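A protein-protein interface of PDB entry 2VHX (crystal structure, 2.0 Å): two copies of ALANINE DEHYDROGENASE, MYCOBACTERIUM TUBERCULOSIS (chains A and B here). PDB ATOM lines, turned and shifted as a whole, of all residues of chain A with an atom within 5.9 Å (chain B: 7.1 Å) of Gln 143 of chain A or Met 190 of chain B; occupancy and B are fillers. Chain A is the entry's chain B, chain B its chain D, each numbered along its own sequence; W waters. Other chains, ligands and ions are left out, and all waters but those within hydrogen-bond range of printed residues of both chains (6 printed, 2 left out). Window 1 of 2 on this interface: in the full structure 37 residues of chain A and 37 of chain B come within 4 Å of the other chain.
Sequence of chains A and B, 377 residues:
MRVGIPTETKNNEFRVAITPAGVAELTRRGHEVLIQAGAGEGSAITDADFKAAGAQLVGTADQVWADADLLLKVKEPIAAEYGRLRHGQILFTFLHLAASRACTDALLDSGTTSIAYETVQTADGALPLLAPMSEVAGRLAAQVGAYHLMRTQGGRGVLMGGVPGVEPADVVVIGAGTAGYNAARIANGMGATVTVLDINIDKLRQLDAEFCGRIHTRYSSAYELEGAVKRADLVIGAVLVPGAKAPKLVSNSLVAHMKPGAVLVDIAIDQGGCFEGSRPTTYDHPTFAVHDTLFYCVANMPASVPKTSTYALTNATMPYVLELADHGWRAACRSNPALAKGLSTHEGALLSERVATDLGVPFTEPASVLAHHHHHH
Met 150 of chain B touches Leu 140 of chain A (SD to CD2, 3.97 Å).
CD1 of Leu 159 of chain B touches CD2 of Leu 140 of chain A, at 3.7 Å.
Met 160 of chain B touches Gln 143 of chain A (CB to NE2, 3.3 Å).
Met 190 of chain B touches Gln 143 of chain A.
CB of Ala 146 of chain A touches OE1 of Gln 143 of chain B, 3.8 Å away.
Tyr 147 of chain A touches Tyr 147 of chain B (CD2 to CG, 3.4 Å).
Gln 143 of chain A touches Ala 146 of chain B, and with the chains exchanged Ala 146 of chain A touches Gln 143 of chain B.
Met 190 of chain B touches its own counterpart, Met 190 of chain A.
11 positions are printed for both chains.
Of the 19 pairs that touch across the chains among the printed residues, 11 have their exchanged pair printed and touching as well.
Of the printed residues of chain B, Arg 139 of chain A touches Leu 159 (3.8 Å), Gly 161 (3.1 Å) and Gly 162 (2.8 Å).
Gln 143 of chain A touches just these residues of chain B: Ala 146 (3.8 Å), Leu 159 (3.8 Å), Met 160 (3.3 Å) and Met 190 (3.4 Å).
Printed residues of chain B within 4 Å of His 148 of chain A: Tyr 147 (3.3 Å).
Of the printed residues of chain A, Tyr 147 of chain B touches Tyr 147 (3.4 Å) and His 148 (3.3 Å).
Printed residues of chain A within 4 Å of Gly 161 of chain B: Arg 139.
Of the printed residues of chain A, Ile 186 of chain B touches Met 190 (3.5 Å).
Met 190 of chain B touches just these residues of chain A: Gln 143 (3.4 Å), Ile 186 (3.5 Å) and Met 190 (3.4 Å).
The nearest residue of chain A that does not touch Met 190 of chain B is Gly 189 of chain A (4.2 Å).
Water W3 bridges O of Gln 143 of chain B and O of Gln 143 of chain A.
Water W5 lies within hydrogen-bond range of NE2 of Gln 143 of chain B (2.7 Å) and O of Met 190 of chain A (2.9 Å).
Water W6 bridges the backbone carbonyl oxygen (O) of Ala 146 of chain A and the side-chain amide oxygen (OE1) of Gln 143 of chain B.
Water W4 bridges the guanidinium group (NH1) of Arg 139 of chain A and the backbone carbonyl oxygen (O) of Gly 161 of chain B.
The backbone NH (N) of Gly 161 of chain B sits close to the backbone carbonyl oxygen (O) of Met 190 of chain B (3.4 Å).
NH1 of Arg 139 of chain A is in hydrogen-bond range of O of Gly 162 of chain B, 2.8 Å away.
A ring nitrogen (NE2) of His 148 of chain A is in hydrogen-bond range of the side-chain hydroxyl (OH) of Tyr 147 of chain B.
The side-chain hydroxyl (OH) of Tyr 147 of chain A sits at hydrogen-bond distance from a ring nitrogen (NE2) of His 148 of chain B (2.9 Å).
The backbone carbonyl oxygen of Gly 161 of chain B sits at hydrogen-bond distance from the guanidinium group of Arg 139 of chain A, 3.1 Å away.
Of the 14 printed residues of chain A, 9 touch a printed residue of chain B.
Hydrophobic or aromatic side chains of chain A that line the printed part of chain B: Leu 140, Ala 146, Tyr 147, His 148, Ile 186 and Met 190.
Among the printed residues, 19 pairs touch across the chains.
Among the printed residues, no Asp or Glu carboxylate lies within 4 Å of a Lys or Arg side-chain nitrogen of the other chain.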
ATOM      1  N   GLY A 138     -17.647  -2.533  25.801  1.00  0.00           N
ATOM      2  CA  GLY A 138     -18.060  -1.596  24.755  1.00  0.00           C
ATOM      3  C   GLY A 138     -19.550  -1.743  24.500  1.00  0.00           C
ATOM      4  O   GLY A 138     -20.256  -0.745  24.426  1.00  0.00           O
ATOM      5  N   ARG A 139     -20.039  -2.965  24.293  1.00  0.00           N
ATOM      6  CA  ARG A 139     -21.449  -3.137  23.996  1.00  0.00           C
ATOM      7  C   ARG A 139     -22.335  -2.647  25.134  1.00  0.00           C
ATOM      8  O   ARG A 139     -23.352  -1.980  24.913  1.00  0.00           O
ATOM      9  CB  ARG A 139     -21.745  -4.577  23.617  1.00  0.00           C
ATOM     10  CG  ARG A 139     -21.025  -4.988  22.314  1.00  0.00           C
ATOM     11  CD  ARG A 139     -21.581  -6.253  21.729  1.00  0.00           C
ATOM     12  NE  ARG A 139     -20.893  -6.544  20.461  1.00  0.00           N
ATOM     13  CZ  ARG A 139     -21.285  -7.465  19.589  1.00  0.00           C
ATOM     14  NH1 ARG A 139     -22.358  -8.242  19.851  1.00  0.00           N
ATOM     15  NH2 ARG A 139     -20.560  -7.657  18.487  1.00  0.00           N
ATOM     16  N   LEU A 140     -21.920  -2.923  26.374  1.00  0.00           N
ATOM     17  CA  LEU A 140     -22.652  -2.438  27.531  1.00  0.00           C
ATOM     18  C   LEU A 140     -22.712  -0.951  27.604  1.00  0.00           C
ATOM     19  O   LEU A 140     -23.718  -0.411  28.063  1.00  0.00           O
ATOM     20  CB  LEU A 140     -21.927  -2.869  28.811  1.00  0.00           C
ATOM     21  CG  LEU A 140     -22.418  -4.174  29.328  1.00  0.00           C
ATOM     22  CD1 LEU A 140     -21.575  -4.499  30.609  1.00  0.00           C
ATOM     23  CD2 LEU A 140     -23.914  -4.026  29.611  1.00  0.00           C
ATOM     24  N   ALA A 141     -21.623  -0.274  27.215  1.00  0.00           N
ATOM     25  CA  ALA A 141     -21.558   1.194  27.322  1.00  0.00           C
ATOM     26  C   ALA A 141     -22.669   1.930  26.509  1.00  0.00           C
ATOM     27  O   ALA A 141     -23.258   2.937  26.943  1.00  0.00           O
ATOM     28  CB  ALA A 141     -20.159   1.673  26.909  1.00  0.00           C
ATOM     29  N   ALA A 142     -22.918   1.423  25.305  1.00  0.00           N
ATOM     30  CA  ALA A 142     -24.052   1.810  24.497  1.00  0.00           C
ATOM     31  C   ALA A 142     -25.360   1.599  25.249  1.00  0.00           C
ATOM     32  O   ALA A 142     -26.195   2.485  25.225  1.00  0.00           O
ATOM     33  CB  ALA A 142     -24.060   1.004  23.256  1.00  0.00           C
ATOM     34  N   GLN A 143     -25.534   0.457  25.943  1.00  0.00           N
ATOM     35  CA  GLN A 143     -26.845   0.182  26.562  1.00  0.00           C
ATOM     36  C   GLN A 143     -27.063   1.025  27.840  1.00  0.00           C
ATOM     37  O   GLN A 143     -28.161   1.557  28.063  1.00  0.00           O
ATOM     38  CB  GLN A 143     -27.007  -1.306  26.928  1.00  0.00           C
ATOM     39  CG  GLN A 143     -26.809  -2.225  25.708  1.00  0.00           C
ATOM     40  CD  GLN A 143     -26.948  -3.681  26.072  1.00  0.00           C
ATOM     41  OE1 GLN A 143     -27.213  -4.032  27.253  1.00  0.00           O
ATOM     42  NE2 GLN A 143     -26.798  -4.541  25.073  1.00  0.00           N
ATOM     43  N   VAL A 144     -26.032   1.113  28.680  1.00  0.00           N
ATOM     44  CA  VAL A 144     -26.150   1.964  29.863  1.00  0.00           C
ATOM     45  C   VAL A 144     -26.218   3.461  29.499  1.00  0.00           C
ATOM     46  O   VAL A 144     -26.900   4.227  30.182  1.00  0.00           O
ATOM     47  CB  VAL A 144     -25.057   1.672  30.925  1.00  0.00           C
ATOM     48  CG1 VAL A 144     -25.015   0.139  31.209  1.00  0.00           C
ATOM     49  CG2 VAL A 144     -23.669   2.195  30.462  1.00  0.00           C
ATOM     50  N   GLY A 145     -25.497   3.857  28.450  1.00  0.00           N
ATOM     51  CA  GLY A 145     -25.554   5.236  27.953  1.00  0.00           C
ATOM     52  C   GLY A 145     -26.987   5.573  27.579  1.00  0.00           C
ATOM     53  O   GLY A 145     -27.512   6.616  27.990  1.00  0.00           O
ATOM     54  N   ALA A 146     -27.634   4.667  26.858  1.00  0.00           N
ATOM     55  CA  ALA A 146     -29.038   4.841  26.441  1.00  0.00           C
ATOM     56  C   ALA A 146     -29.972   5.037  27.603  1.00  0.00           C
ATOM     57  O   ALA A 146     -30.884   5.900  27.556  1.00  0.00           O
ATOM     58  CB  ALA A 146     -29.501   3.649  25.601  1.00  0.00           C
ATOM     59  N   TYR A 147     -29.780   4.206  28.631  1.00  0.00           N
ATOM     60  CA  TYR A 147     -30.613   4.226  29.806  1.00  0.00           C
ATOM     61  C   TYR A 147     -30.472   5.507  30.631  1.00  0.00           C
ATOM     62  O   TYR A 147     -31.481   6.077  31.053  1.00  0.00           O
ATOM     63  CB  TYR A 147     -30.300   3.013  30.695  1.00  0.00           C
ATOM     64  CG  TYR A 147     -31.401   2.714  31.707  1.00  0.00           C
ATOM     65  CD1 TYR A 147     -31.294   3.157  33.028  1.00  0.00           C
ATOM     66  CD2 TYR A 147     -32.539   1.988  31.342  1.00  0.00           C
ATOM     67  CE1 TYR A 147     -32.297   2.895  33.952  1.00  0.00           C
ATOM     68  CE2 TYR A 147     -33.535   1.704  32.281  1.00  0.00           C
ATOM     69  CZ  TYR A 147     -33.408   2.164  33.560  1.00  0.00           C
ATOM     70  OH  TYR A 147     -34.414   1.879  34.481  1.00  0.00           O
ATOM     71  N   HIS A 148     -29.237   5.939  30.892  1.00  0.00           N
ATOM     72  CA  HIS A 148     -29.002   7.156  31.663  1.00  0.00           C
ATOM     73  C   HIS A 148     -29.249   8.441  30.868  1.00  0.00           C
ATOM     74  O   HIS A 148     -29.359   9.487  31.442  1.00  0.00           O
ATOM     75  CB  HIS A 148     -27.611   7.101  32.247  1.00  0.00           C
ATOM     76  CG  HIS A 148     -27.464   6.021  33.285  1.00  0.00           C
ATOM     77  ND1 HIS A 148     -27.913   6.172  34.585  1.00  0.00           N
ATOM     78  CD2 HIS A 148     -26.986   4.757  33.195  1.00  0.00           C
ATOM     79  CE1 HIS A 148     -27.670   5.059  35.266  1.00  0.00           C
ATOM     80  NE2 HIS A 148     -27.121   4.181  34.439  1.00  0.00           N
ATOM     81  N   ILE A 186     -23.194  -0.975  18.643  1.00  0.00           N
ATOM     82  CA  ILE A 186     -24.475  -1.109  19.259  1.00  0.00           C
ATOM     83  C   ILE A 186     -25.214   0.231  19.232  1.00  0.00           C
ATOM     84  O   ILE A 186     -26.433   0.287  19.005  1.00  0.00           O
ATOM     85  CB  ILE A 186     -24.312  -1.630  20.731  1.00  0.00           C
ATOM     86  CG1 ILE A 186     -23.720  -3.046  20.762  1.00  0.00           C
ATOM     87  CG2 ILE A 186     -25.650  -1.644  21.437  1.00  0.00           C
ATOM     88  CD1 ILE A 186     -24.329  -4.133  19.789  1.00  0.00           C
ATOM     89  N   GLY A 189     -26.759   0.570  15.987  1.00  0.00           N
ATOM     90  CA  GLY A 189     -27.877  -0.360  15.803  1.00  0.00           C
ATOM     91  C   GLY A 189     -29.103   0.135  16.550  1.00  0.00           C
ATOM     92  O   GLY A 189     -30.245  -0.274  16.247  1.00  0.00           O
ATOM     93  N   MET A 190     -28.899   1.024  17.525  1.00  0.00           N
ATOM     94  CA  MET A 190     -30.028   1.472  18.332  1.00  0.00           C
ATOM     95  C   MET A 190     -30.626   2.691  17.618  1.00  0.00           C
ATOM     96  O   MET A 190     -31.611   3.256  18.076  1.00  0.00           O
ATOM     97  CB  MET A 190     -29.629   1.845  19.763  1.00  0.00           C
ATOM     98  CG  MET A 190     -29.228   0.637  20.611  1.00  0.00           C
ATOM     99  SD  MET A 190     -28.591   1.089  22.240  1.00  0.00           S
ATOM    100  CE  MET A 190     -30.147   1.338  23.130  1.00  0.00           C
ATOM    101  N   ARG B 139     -39.533   1.619  21.091  1.00  0.00           N
ATOM    102  CA  ARG B 139     -38.064   1.749  21.077  1.00  0.00           C
ATOM    103  C   ARG B 139     -37.488   1.731  22.489  1.00  0.00           C
ATOM    104  O   ARG B 139     -36.470   1.070  22.757  1.00  0.00           O
ATOM    105  CB  ARG B 139     -37.644   3.025  20.359  1.00  0.00           C
ATOM    106  CG  ARG B 139     -38.077   3.016  18.864  1.00  0.00           C
ATOM    107  CD  ARG B 139     -37.381   3.990  18.026  1.00  0.00           C
ATOM    108  NE  ARG B 139     -37.852   3.753  16.656  1.00  0.00           N
ATOM    109  CZ  ARG B 139     -37.294   4.212  15.545  1.00  0.00           C
ATOM    110  NH1 ARG B 139     -36.225   5.018  15.601  1.00  0.00           N
ATOM    111  NH2 ARG B 139     -37.857   3.920  14.360  1.00  0.00           N
ATOM    112  N   ALA B 142     -37.133  -1.851  24.290  1.00  0.00           N
ATOM    113  CA  ALA B 142     -35.893  -2.549  23.970  1.00  0.00           C
ATOM    114  C   ALA B 142     -34.692  -2.052  24.853  1.00  0.00           C
ATOM    115  O   ALA B 142     -34.021  -2.873  25.518  1.00  0.00           O
ATOM    116  CB  ALA B 142     -35.585  -2.467  22.446  1.00  0.00           C
ATOM    117  N   GLN B 143     -34.504  -0.724  24.940  1.00  0.00           N
ATOM    118  CA  GLN B 143     -33.432  -0.109  25.734  1.00  0.00           C
ATOM    119  C   GLN B 143     -33.553  -0.531  27.199  1.00  0.00           C
ATOM    120  O   GLN B 143     -32.564  -0.828  27.854  1.00  0.00           O
ATOM    121  CB  GLN B 143     -33.519   1.422  25.642  1.00  0.00           C
ATOM    122  CG  GLN B 143     -33.489   1.912  24.138  1.00  0.00           C
ATOM    123  CD  GLN B 143     -33.186   3.388  23.961  1.00  0.00           C
ATOM    124  OE1 GLN B 143     -33.178   4.166  24.930  1.00  0.00           O
ATOM    125  NE2 GLN B 143     -32.966   3.789  22.705  1.00  0.00           N
ATOM    126  N   VAL B 144     -34.777  -0.489  27.699  1.00  0.00           N
ATOM    127  CA  VAL B 144     -35.085  -0.725  29.085  1.00  0.00           C
ATOM    128  C   VAL B 144     -34.991  -2.200  29.465  1.00  0.00           C
ATOM    129  O   VAL B 144     -34.578  -2.559  30.601  1.00  0.00           O
ATOM    130  CB  VAL B 144     -36.483  -0.142  29.330  1.00  0.00           C
ATOM    131  CG1 VAL B 144     -37.137  -0.823  30.436  1.00  0.00           C
ATOM    132  CG2 VAL B 144     -36.384   1.376  29.555  1.00  0.00           C
ATOM    133  N   GLY B 145     -35.361  -3.080  28.530  1.00  0.00           N
ATOM    134  CA  GLY B 145     -35.320  -4.539  28.801  1.00  0.00           C
ATOM    135  C   GLY B 145     -33.866  -4.991  28.877  1.00  0.00           C
ATOM    136  O   GLY B 145     -33.466  -5.779  29.784  1.00  0.00           O
ATOM    137  N   ALA B 146     -33.063  -4.396  28.003  1.00  0.00           N
ATOM    138  CA  ALA B 146     -31.622  -4.651  27.925  1.00  0.00           C
ATOM    139  C   ALA B 146     -30.936  -4.275  29.197  1.00  0.00           C
ATOM    140  O   ALA B 146     -30.014  -4.961  29.610  1.00  0.00           O
ATOM    141  CB  ALA B 146     -31.004  -3.861  26.865  1.00  0.00           C
ATOM    142  N   TYR B 147     -31.309  -3.131  29.744  1.00  0.00           N
ATOM    143  CA  TYR B 147     -30.681  -2.632  30.971  1.00  0.00           C
ATOM    144  C   TYR B 147     -31.079  -3.511  32.114  1.00  0.00           C
ATOM    145  O   TYR B 147     -30.275  -3.820  32.985  1.00  0.00           O
ATOM    146  CB  TYR B 147     -31.153  -1.218  31.247  1.00  0.00           C
ATOM    147  CG  TYR B 147     -30.434  -0.530  32.362  1.00  0.00           C
ATOM    148  CD1 TYR B 147     -30.958  -0.545  33.680  1.00  0.00           C
ATOM    149  CD2 TYR B 147     -29.199   0.075  32.136  1.00  0.00           C
ATOM    150  CE1 TYR B 147     -30.290   0.090  34.732  1.00  0.00           C
ATOM    151  CE2 TYR B 147     -28.519   0.726  33.179  1.00  0.00           C
ATOM    152  CZ  TYR B 147     -29.064   0.694  34.479  1.00  0.00           C
ATOM    153  OH  TYR B 147     -28.391   1.348  35.491  1.00  0.00           O
ATOM    154  N   HIS B 148     -32.336  -3.906  32.131  1.00  0.00           N
ATOM    155  CA  HIS B 148     -32.833  -4.722  33.244  1.00  0.00           C
ATOM    156  C   HIS B 148     -32.446  -6.227  33.234  1.00  0.00           C
ATOM    157  O   HIS B 148     -32.415  -6.904  34.291  1.00  0.00           O
ATOM    158  CB  HIS B 148     -34.340  -4.454  33.484  1.00  0.00           C
ATOM    159  CG  HIS B 148     -34.601  -3.099  34.094  1.00  0.00           C
ATOM    160  ND1 HIS B 148     -34.498  -2.853  35.454  1.00  0.00           N
ATOM    161  CD2 HIS B 148     -34.894  -1.900  33.520  1.00  0.00           C
ATOM    162  CE1 HIS B 148     -34.732  -1.571  35.691  1.00  0.00           C
ATOM    163  NE2 HIS B 148     -34.975  -0.971  34.534  1.00  0.00           N
ATOM    164  N   LEU B 149     -32.099  -6.739  32.069  1.00  0.00           N
ATOM    165  CA  LEU B 149     -31.351  -7.989  31.970  1.00  0.00           C
ATOM    166  C   LEU B 149     -29.947  -8.032  32.641  1.00  0.00           C
ATOM    167  O   LEU B 149     -29.348  -9.077  32.655  1.00  0.00           O
ATOM    168  CB  LEU B 149     -31.175  -8.362  30.494  1.00  0.00           C
ATOM    169  CG  LEU B 149     -32.356  -9.092  29.859  1.00  0.00           C
ATOM    170  CD1 LEU B 149     -32.159  -9.163  28.310  1.00  0.00           C
ATOM    171  CD2 LEU B 149     -32.477 -10.482  30.357  1.00  0.00           C
ATOM    172  N   MET B 150     -29.388  -6.926  33.124  1.00  0.00           N
ATOM    173  CA  MET B 150     -28.081  -6.962  33.721  1.00  0.00           C
ATOM    174  C   MET B 150     -28.377  -7.577  35.105  1.00  0.00           C
ATOM    175  O   MET B 150     -29.457  -7.333  35.651  1.00  0.00           O
ATOM    176  CB  MET B 150     -27.491  -5.555  33.831  1.00  0.00           C
ATOM    177  CG  MET B 150     -27.248  -4.863  32.347  1.00  0.00           C
ATOM    178  SD  MET B 150     -26.320  -3.351  32.690  1.00  0.00           S
ATOM    179  CE  MET B 150     -27.423  -2.549  33.782  1.00  0.00           C
ATOM    180  N   VAL B 158     -27.584 -11.180  30.961  1.00  0.00           N
ATOM    181  CA  VAL B 158     -27.331 -11.460  29.558  1.00  0.00           C
ATOM    182  C   VAL B 158     -27.217 -10.166  28.744  1.00  0.00           C
ATOM    183  O   VAL B 158     -28.110  -9.333  28.757  1.00  0.00           O
ATOM    184  CB  VAL B 158     -28.471 -12.347  28.986  1.00  0.00           C
ATOM    185  CG1 VAL B 158     -28.224 -12.694  27.555  1.00  0.00           C
ATOM    186  CG2 VAL B 158     -28.607 -13.644  29.824  1.00  0.00           C
ATOM    187  N   LEU B 159     -26.118 -10.011  28.019  1.00  0.00           N
ATOM    188  CA  LEU B 159     -25.964  -8.892  27.096  1.00  0.00           C
ATOM    189  C   LEU B 159     -26.874  -9.095  25.895  1.00  0.00           C
ATOM    190  O   LEU B 159     -26.950 -10.212  25.334  1.00  0.00           O
ATOM    191  CB  LEU B 159     -24.496  -8.814  26.655  1.00  0.00           C
ATOM    192  CG  LEU B 159     -23.980  -7.616  25.830  1.00  0.00           C
ATOM    193  CD1 LEU B 159     -23.971  -6.373  26.761  1.00  0.00           C
ATOM    194  CD2 LEU B 159     -22.557  -7.897  25.317  1.00  0.00           C
ATOM    195  N   MET B 160     -27.521  -8.019  25.429  1.00  0.00           N
ATOM    196  CA  MET B 160     -28.480  -8.123  24.302  1.00  0.00           C
ATOM    197  C   MET B 160     -27.883  -8.813  23.108  1.00  0.00           C
ATOM    198  O   MET B 160     -28.467  -9.726  22.553  1.00  0.00           O
ATOM    199  CB  MET B 160     -29.022  -6.742  23.888  1.00  0.00           C
ATOM    200  CG  MET B 160     -30.144  -6.182  24.672  1.00  0.00           C
ATOM    201  SD  MET B 160     -31.715  -7.023  24.514  1.00  0.00           S
ATOM    202  CE  MET B 160     -32.816  -5.932  23.598  1.00  0.00           C
ATOM    203  N   GLY B 161     -26.732  -8.339  22.650  1.00  0.00           N
ATOM    204  CA  GLY B 161     -26.133  -8.900  21.490  1.00  0.00           C
ATOM    205  C   GLY B 161     -25.101  -9.977  21.619  1.00  0.00           C
ATOM    206  O   GLY B 161     -24.531 -10.345  20.621  1.00  0.00           O
ATOM    207  N   GLY B 162     -24.859 -10.527  22.828  1.00  0.00           N
ATOM    208  CA  GLY B 162     -23.688 -11.378  23.009  1.00  0.00           C
ATOM    209  C   GLY B 162     -22.446 -10.685  22.459  1.00  0.00           C
ATOM    210  O   GLY B 162     -22.396  -9.463  22.324  1.00  0.00           O
ATOM    211  N   PRO B 168     -26.340 -14.440  21.962  1.00  0.00           N
ATOM    212  CA  PRO B 168     -27.078 -13.189  22.269  1.00  0.00           C
ATOM    213  C   PRO B 168     -28.357 -13.450  23.044  1.00  0.00           C
ATOM    214  O   PRO B 168     -28.788 -14.572  23.085  1.00  0.00           O
ATOM    215  CB  PRO B 168     -27.482 -12.669  20.892  1.00  0.00           C
ATOM    216  CG  PRO B 168     -27.368 -13.793  20.045  1.00  0.00           C
ATOM    217  CD  PRO B 168     -26.338 -14.724  20.515  1.00  0.00           C
ATOM    218  N   ALA B 184     -39.114  -4.529  18.279  1.00  0.00           N
ATOM    219  CA  ALA B 184     -38.335  -5.540  17.549  1.00  0.00           C
ATOM    220  C   ALA B 184     -37.165  -4.942  16.777  1.00  0.00           C
ATOM    221  O   ALA B 184     -36.089  -5.509  16.771  1.00  0.00           O
ATOM    222  CB  ALA B 184     -39.234  -6.339  16.614  1.00  0.00           C
ATOM    223  N   ARG B 185     -37.372  -3.792  16.140  1.00  0.00           N
ATOM    224  CA  ARG B 185     -36.326  -3.197  15.330  1.00  0.00           C
ATOM    225  C   ARG B 185     -35.155  -2.778  16.199  1.00  0.00           C
ATOM    226  O   ARG B 185     -33.989  -2.976  15.809  1.00  0.00           O
ATOM    227  CB  ARG B 185     -36.869  -2.008  14.525  1.00  0.00           C
ATOM    228  CG  ARG B 185     -36.069  -0.774  14.711  1.00  0.00           C
ATOM    229  CD  ARG B 185     -35.580  -0.130  13.415  1.00  0.00           C
ATOM    230  NE  ARG B 185     -36.656   0.397  12.600  1.00  0.00           N
ATOM    231  CZ  ARG B 185     -36.604   1.521  11.866  1.00  0.00           C
ATOM    232  NH1 ARG B 185     -35.521   2.320  11.819  1.00  0.00           N
ATOM    233  NH2 ARG B 185     -37.685   1.851  11.179  1.00  0.00           N
ATOM    234  N   ILE B 186     -35.443  -2.189  17.363  1.00  0.00           N
ATOM    235  CA  ILE B 186     -34.340  -1.705  18.196  1.00  0.00           C
ATOM    236  C   ILE B 186     -33.655  -2.899  18.914  1.00  0.00           C
ATOM    237  O   ILE B 186     -32.432  -2.944  18.975  1.00  0.00           O
ATOM    238  CB  ILE B 186     -34.753  -0.594  19.235  1.00  0.00           C
ATOM    239  CG1 ILE B 186     -35.246   0.684  18.549  1.00  0.00           C
ATOM    240  CG2 ILE B 186     -33.584  -0.312  20.246  1.00  0.00           C
ATOM    241  CD1 ILE B 186     -34.371   1.258  17.410  1.00  0.00           C
ATOM    242  N   ALA B 187     -34.427  -3.888  19.363  1.00  0.00           N
ATOM    243  CA  ALA B 187     -33.822  -5.106  19.962  1.00  0.00           C
ATOM    244  C   ALA B 187     -32.905  -5.823  18.993  1.00  0.00           C
ATOM    245  O   ALA B 187     -31.791  -6.287  19.353  1.00  0.00           O
ATOM    246  CB  ALA B 187     -34.893  -6.050  20.466  1.00  0.00           C
ATOM    247  N   ASN B 188     -33.346  -5.871  17.740  1.00  0.00           N
ATOM    248  CA  ASN B 188     -32.538  -6.424  16.658  1.00  0.00           C
ATOM    249  C   ASN B 188     -31.274  -5.613  16.384  1.00  0.00           C
ATOM    250  O   ASN B 188     -30.191  -6.201  16.251  1.00  0.00           O
ATOM    251  CB  ASN B 188     -33.408  -6.513  15.384  1.00  0.00           C
ATOM    252  CG  ASN B 188     -32.682  -7.132  14.211  1.00  0.00           C
ATOM    253  OD1 ASN B 188     -32.352  -8.329  14.215  1.00  0.00           O
ATOM    254  ND2 ASN B 188     -32.477  -6.341  13.155  1.00  0.00           N
ATOM    255  N   GLY B 189     -31.403  -4.276  16.168  1.00  0.00           N
ATOM    256  CA  GLY B 189     -30.207  -3.432  15.952  1.00  0.00           C
ATOM    257  C   GLY B 189     -29.196  -3.552  17.121  1.00  0.00           C
ATOM    258  O   GLY B 189     -28.004  -3.270  16.976  1.00  0.00           O
ATOM    259  N   MET B 190     -29.687  -3.942  18.282  1.00  0.00           N
ATOM    260  CA  MET B 190     -28.814  -4.230  19.428  1.00  0.00           C
ATOM    261  C   MET B 190     -28.139  -5.647  19.412  1.00  0.00           C
ATOM    262  O   MET B 190     -27.300  -5.937  20.257  1.00  0.00           O
ATOM    263  CB  MET B 190     -29.600  -4.070  20.726  1.00  0.00           C
ATOM    264  CG  MET B 190     -30.089  -2.626  21.047  1.00  0.00           C
ATOM    265  SD  MET B 190     -30.977  -2.492  22.664  1.00  0.00           S
ATOM    266  CE  MET B 190     -29.533  -2.234  23.668  1.00  0.00           C
ATOM    267  N   GLY B 191     -28.418  -6.435  18.361  1.00  0.00           N
ATOM    268  CA  GLY B 191     -27.845  -7.753  18.132  1.00  0.00           C
ATOM    269  C   GLY B 191     -28.551  -8.921  18.849  1.00  0.00           C
ATOM    270  O   GLY B 191     -28.089 -10.061  18.805  1.00  0.00           O
ATOM    271  N   ALA B 192     -29.695  -8.667  19.449  1.00  0.00           N
ATOM    272  CA  ALA B 192     -30.497  -9.736  20.090  1.00  0.00           C
ATOM    273  C   ALA B 192     -31.116 -10.627  18.999  1.00  0.00           C
ATOM    274  O   ALA B 192     -31.309 -10.187  17.865  1.00  0.00           O
ATOM    275  CB  ALA B 192     -31.613  -9.117  20.932  1.00  0.00           C
ATOM    276  N   THR B 193     -31.445 -11.861  19.340  1.00  0.00           N
ATOM    277  CA  THR B 193     -32.235 -12.669  18.429  1.00  0.00           C
ATOM    278  C   THR B 193     -33.701 -12.437  18.718  1.00  0.00           C
ATOM    279  O   THR B 193     -34.207 -12.763  19.817  1.00  0.00           O
ATOM    280  CB  THR B 193     -31.864 -14.138  18.545  1.00  0.00           C
ATOM    281  OG1 THR B 193     -30.467 -14.268  18.245  1.00  0.00           O
ATOM    282  CG2 THR B 193     -32.671 -14.970  17.556  1.00  0.00           C
ATOM    283  N   ARG B 214     -34.411 -11.480   9.056  1.00  0.00           N
ATOM    284  CA  ARG B 214     -33.581 -11.363  10.224  1.00  0.00           C
ATOM    285  C   ARG B 214     -34.428 -11.356  11.525  1.00  0.00           C
ATOM    286  O   ARG B 214     -34.057 -11.984  12.523  1.00  0.00           O
ATOM    287  CB  ARG B 214     -32.662 -10.159  10.157  1.00  0.00           C
ATOM    288  CG  ARG B 214     -31.973  -9.987  11.521  1.00  0.00           C
ATOM    289  CD  ARG B 214     -30.663  -9.230  11.461  1.00  0.00           C
ATOM    290  NE  ARG B 214     -29.969  -9.403  12.725  1.00  0.00           N
ATOM    291  CZ  ARG B 214     -28.724  -9.001  12.953  1.00  0.00           C
ATOM    292  NH1 ARG B 214     -28.030  -8.436  11.952  1.00  0.00           N
ATOM    293  NH2 ARG B 214     -28.158  -9.200  14.165  1.00  0.00           N
HETATM  294  O   HOH W   1     -33.427   4.077  27.465  1.00  0.00           O
HETATM  295  O   HOH W   2     -25.663  -5.694  22.850  1.00  0.00           O
HETATM  296  O   HOH W   3     -30.377   0.174  27.003  1.00  0.00           O
HETATM  297  O   HOH W   4     -21.923 -11.318  18.650  1.00  0.00           O
HETATM  298  O   HOH W   5     -33.579   3.974  20.041  1.00  0.00           O
HETATM  299  O   HOH W   6     -32.015   6.798  25.222  1.00  0.00           O
